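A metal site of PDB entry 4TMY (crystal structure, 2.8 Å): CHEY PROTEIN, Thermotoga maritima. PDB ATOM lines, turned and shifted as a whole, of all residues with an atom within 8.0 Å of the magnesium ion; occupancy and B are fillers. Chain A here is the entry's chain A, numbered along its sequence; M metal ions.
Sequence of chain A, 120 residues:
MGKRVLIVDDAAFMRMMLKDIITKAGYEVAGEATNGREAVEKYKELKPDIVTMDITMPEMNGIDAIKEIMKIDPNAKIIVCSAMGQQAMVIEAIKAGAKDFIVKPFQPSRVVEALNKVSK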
ATOM      1  N   VAL A   8      29.633  15.099  10.948  1.00  0.00           N
ATOM      2  CA  VAL A   8      28.602  14.863   9.934  1.00  0.00           C
ATOM      3  C   VAL A   8      29.087  15.375   8.557  1.00  0.00           C
ATOM      4  O   VAL A   8      29.430  16.553   8.384  1.00  0.00           O
ATOM      5  CB  VAL A   8      27.296  15.548  10.301  1.00  0.00           C
ATOM      6  CG1 VAL A   8      26.111  14.820   9.681  1.00  0.00           C
ATOM      7  CG2 VAL A   8      27.122  15.600  11.811  1.00  0.00           C
ATOM      8  N   ASP A   9      29.163  14.470   7.596  1.00  0.00           N
ATOM      9  CA  ASP A   9      29.569  14.755   6.217  1.00  0.00           C
ATOM     10  C   ASP A   9      29.321  13.513   5.407  1.00  0.00           C
ATOM     11  O   ASP A   9      29.708  12.424   5.798  1.00  0.00           O
ATOM     12  CB  ASP A   9      31.025  15.233   6.051  1.00  0.00           C
ATOM     13  CG  ASP A   9      31.345  15.697   4.648  1.00  0.00           C
ATOM     14  OD1 ASP A   9      30.810  15.253   3.646  1.00  0.00           O
ATOM     15  OD2 ASP A   9      32.242  16.654   4.618  1.00  0.00           O
ATOM     16  N   ASP A  10      28.646  13.716   4.273  1.00  0.00           N
ATOM     17  CA  ASP A  10      28.285  12.626   3.386  1.00  0.00           C
ATOM     18  C   ASP A  10      29.450  12.037   2.613  1.00  0.00           C
ATOM     19  O   ASP A  10      29.328  10.968   2.039  1.00  0.00           O
ATOM     20  CB  ASP A  10      27.037  12.944   2.507  1.00  0.00           C
ATOM     21  CG  ASP A  10      27.277  14.005   1.478  1.00  0.00           C
ATOM     22  OD1 ASP A  10      27.429  15.188   1.751  1.00  0.00           O
ATOM     23  OD2 ASP A  10      27.458  13.503   0.280  1.00  0.00           O
ATOM     24  N   ALA A  11      30.614  12.707   2.668  1.00  0.00           N
ATOM     25  CA  ALA A  11      31.836  12.270   2.012  1.00  0.00           C
ATOM     26  C   ALA A  11      32.853  11.624   2.932  1.00  0.00           C
ATOM     27  O   ALA A  11      33.631  12.331   3.573  1.00  0.00           O
ATOM     28  CB  ALA A  11      32.514  13.474   1.394  1.00  0.00           C
ATOM     29  N   MET A  14      36.063  13.224   3.340  1.00  0.00           N
ATOM     30  CA  MET A  14      35.999  14.485   4.043  1.00  0.00           C
ATOM     31  C   MET A  14      35.985  14.329   5.568  1.00  0.00           C
ATOM     32  O   MET A  14      36.597  15.107   6.333  1.00  0.00           O
ATOM     33  CB  MET A  14      34.890  15.371   3.457  1.00  0.00           C
ATOM     34  CG  MET A  14      35.356  16.783   3.151  1.00  0.00           C
ATOM     35  SD  MET A  14      36.483  16.938   1.742  1.00  0.00           S
ATOM     36  CE  MET A  14      37.875  17.794   2.501  1.00  0.00           C
ATOM     37  N   THR A  34      26.316  10.428   8.507  1.00  0.00           N
ATOM     38  CA  THR A  34      26.408  10.561   7.055  1.00  0.00           C
ATOM     39  C   THR A  34      25.289  11.359   6.407  1.00  0.00           C
ATOM     40  O   THR A  34      25.107  11.295   5.195  1.00  0.00           O
ATOM     41  CB  THR A  34      26.462   9.174   6.433  1.00  0.00           C
ATOM     42  OG1 THR A  34      25.405   8.407   6.960  1.00  0.00           O
ATOM     43  CG2 THR A  34      27.762   8.527   6.821  1.00  0.00           C
ATOM     44  N   MET A  53      29.166  20.345  11.141  1.00  0.00           N
ATOM     45  CA  MET A  53      28.081  19.963  10.252  1.00  0.00           C
ATOM     46  C   MET A  53      28.237  20.325   8.783  1.00  0.00           C
ATOM     47  O   MET A  53      28.343  21.497   8.448  1.00  0.00           O
ATOM     48  CB  MET A  53      26.741  20.439  10.837  1.00  0.00           C
ATOM     49  CG  MET A  53      25.554  20.166   9.952  1.00  0.00           C
ATOM     50  SD  MET A  53      24.848  18.577  10.371  1.00  0.00           S
ATOM     51  CE  MET A  53      24.205  18.907  12.030  1.00  0.00           C
ATOM     52  N   ASP A  54      28.289  19.313   7.932  1.00  0.00           N
ATOM     53  CA  ASP A  54      28.336  19.514   6.500  1.00  0.00           C
ATOM     54  C   ASP A  54      26.997  20.103   6.096  1.00  0.00           C
ATOM     55  O   ASP A  54      25.991  19.837   6.757  1.00  0.00           O
ATOM     56  CB  ASP A  54      28.577  18.198   5.747  1.00  0.00           C
ATOM     57  CG  ASP A  54      28.754  18.409   4.260  1.00  0.00           C
ATOM     58  OD1 ASP A  54      29.314  19.388   3.779  1.00  0.00           O
ATOM     59  OD2 ASP A  54      28.293  17.407   3.536  1.00  0.00           O
ATOM     60  N   ILE A  55      26.974  20.914   5.055  1.00  0.00           N
ATOM     61  CA  ILE A  55      25.721  21.523   4.654  1.00  0.00           C
ATOM     62  C   ILE A  55      24.946  20.695   3.670  1.00  0.00           C
ATOM     63  O   ILE A  55      23.849  20.230   3.961  1.00  0.00           O
ATOM     64  CB  ILE A  55      25.891  22.916   4.130  1.00  0.00           C
ATOM     65  CG1 ILE A  55      26.085  23.876   5.299  1.00  0.00           C
ATOM     66  CG2 ILE A  55      24.655  23.288   3.344  1.00  0.00           C
ATOM     67  CD1 ILE A  55      26.430  25.285   4.848  1.00  0.00           C
ATOM     68  N   THR A  56      25.533  20.499   2.511  1.00  0.00           N
ATOM     69  CA  THR A  56      24.892  19.704   1.466  1.00  0.00           C
ATOM     70  C   THR A  56      24.998  18.202   1.713  1.00  0.00           C
ATOM     71  O   THR A  56      26.057  17.608   1.510  1.00  0.00           O
ATOM     72  CB  THR A  56      25.464  20.036   0.079  1.00  0.00           C
ATOM     73  OG1 THR A  56      25.417  21.443  -0.092  1.00  0.00           O
ATOM     74  CG2 THR A  56      24.635  19.341  -0.998  1.00  0.00           C
ATOM     75  N   MET A  57      23.870  17.605   2.097  1.00  0.00           N
ATOM     76  CA  MET A  57      23.777  16.171   2.349  1.00  0.00           C
ATOM     77  C   MET A  57      22.434  15.647   1.920  1.00  0.00           C
ATOM     78  O   MET A  57      21.453  16.374   1.908  1.00  0.00           O
ATOM     79  CB  MET A  57      24.004  15.825   3.842  1.00  0.00           C
ATOM     80  CG  MET A  57      25.350  16.266   4.377  1.00  0.00           C
ATOM     81  SD  MET A  57      25.465  15.995   6.150  1.00  0.00           S
ATOM     82  CE  MET A  57      24.564  17.443   6.748  1.00  0.00           C
ATOM     83  N   PRO A  58      22.379  14.355   1.651  1.00  0.00           N
ATOM     84  CA  PRO A  58      21.152  13.735   1.227  1.00  0.00           C
ATOM     85  C   PRO A  58      20.165  13.565   2.344  1.00  0.00           C
ATOM     86  O   PRO A  58      20.490  13.793   3.504  1.00  0.00           O
ATOM     87  CB  PRO A  58      21.546  12.374   0.654  1.00  0.00           C
ATOM     88  CG  PRO A  58      23.029  12.464   0.328  1.00  0.00           C
ATOM     89  CD  PRO A  58      23.563  13.706   1.029  1.00  0.00           C
ATOM     90  N   CYS A  81      30.499  23.220   8.148  1.00  0.00           N
ATOM     91  CA  CYS A  81      31.555  23.171   7.121  1.00  0.00           C
ATOM     92  C   CYS A  81      30.974  23.364   5.773  1.00  0.00           C
ATOM     93  O   CYS A  81      30.155  22.557   5.339  1.00  0.00           O
ATOM     94  CB  CYS A  81      32.287  21.834   7.028  1.00  0.00           C
ATOM     95  SG  CYS A  81      32.161  20.888   8.543  1.00  0.00           S
ATOM     96  N   ALA A  83      31.566  24.544   1.536  1.00  0.00           N
ATOM     97  CA  ALA A  83      32.510  24.694   0.462  1.00  0.00           C
ATOM     98  C   ALA A  83      32.510  26.169   0.166  1.00  0.00           C
ATOM     99  O   ALA A  83      31.577  26.872   0.529  1.00  0.00           O
ATOM    100  CB  ALA A  83      32.078  23.987  -0.791  1.00  0.00           C
ATOM    101  N   GLN A  86      29.468  28.963  -0.807  1.00  0.00           N
ATOM    102  CA  GLN A  86      28.260  28.505  -0.107  1.00  0.00           C
ATOM    103  C   GLN A  86      27.914  29.494   1.028  1.00  0.00           C
ATOM    104  O   GLN A  86      27.188  29.171   1.981  1.00  0.00           O
ATOM    105  CB  GLN A  86      28.444  27.121   0.494  1.00  0.00           C
ATOM    106  CG  GLN A  86      27.927  26.022  -0.443  1.00  0.00           C
ATOM    107  CD  GLN A  86      27.928  24.672   0.246  1.00  0.00           C
ATOM    108  OE1 GLN A  86      28.979  24.120   0.591  1.00  0.00           O
ATOM    109  NE2 GLN A  86      26.732  24.180   0.504  1.00  0.00           N
ATOM    110  N   LYS A 104      35.968  24.026   3.403  1.00  0.00           N
ATOM    111  CA  LYS A 104      36.505  22.835   2.756  1.00  0.00           C
ATOM    112  C   LYS A 104      37.222  23.273   1.483  1.00  0.00           C
ATOM    113  O   LYS A 104      36.708  24.107   0.729  1.00  0.00           O
ATOM    114  CB  LYS A 104      35.397  21.883   2.366  1.00  0.00           C
ATOM    115  CG  LYS A 104      34.849  21.154   3.557  1.00  0.00           C
ATOM    116  CD  LYS A 104      33.342  20.966   3.469  1.00  0.00           C
ATOM    117  CE  LYS A 104      32.985  19.653   2.831  1.00  0.00           C
ATOM    118  NZ  LYS A 104      31.916  18.989   3.569  1.00  0.00           N
HETATM  119 MG    MG M   1      28.350  17.374   1.418  1.00  0.00          MG
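The side-chain carboxylate of Asp 9 is in hydrogen-bond range of the backbone NH of Ala 11 (2.7 Å). OD1 of Asp 54 lies within salt-bridge range of NZ of Lys 104 (2.6 Å). The side-chain hydroxyl of Thr 56 lies within hydrogen-bond range of the side-chain amide nitrogen of Gln 86, 3.1 Å away. The backbone NH (N) of Asp 54 is in hydrogen-bond range of the backbone carbonyl oxygen (O) of Val 8 (3.0 Å). The side-chain amino group of Lys 104 lies within salt-bridge range of the side-chain carboxylate of Asp 9 (2.6 Å).
Asp 9 touches the magnesium ion (OD1 to MG, 3.9 Å).
The magnesium ion is bound by OD2 of Asp 54 (2.1 Å), O of Thr 56 (2.3 Å) and OD1 of Asp 10 (2.4 Å).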
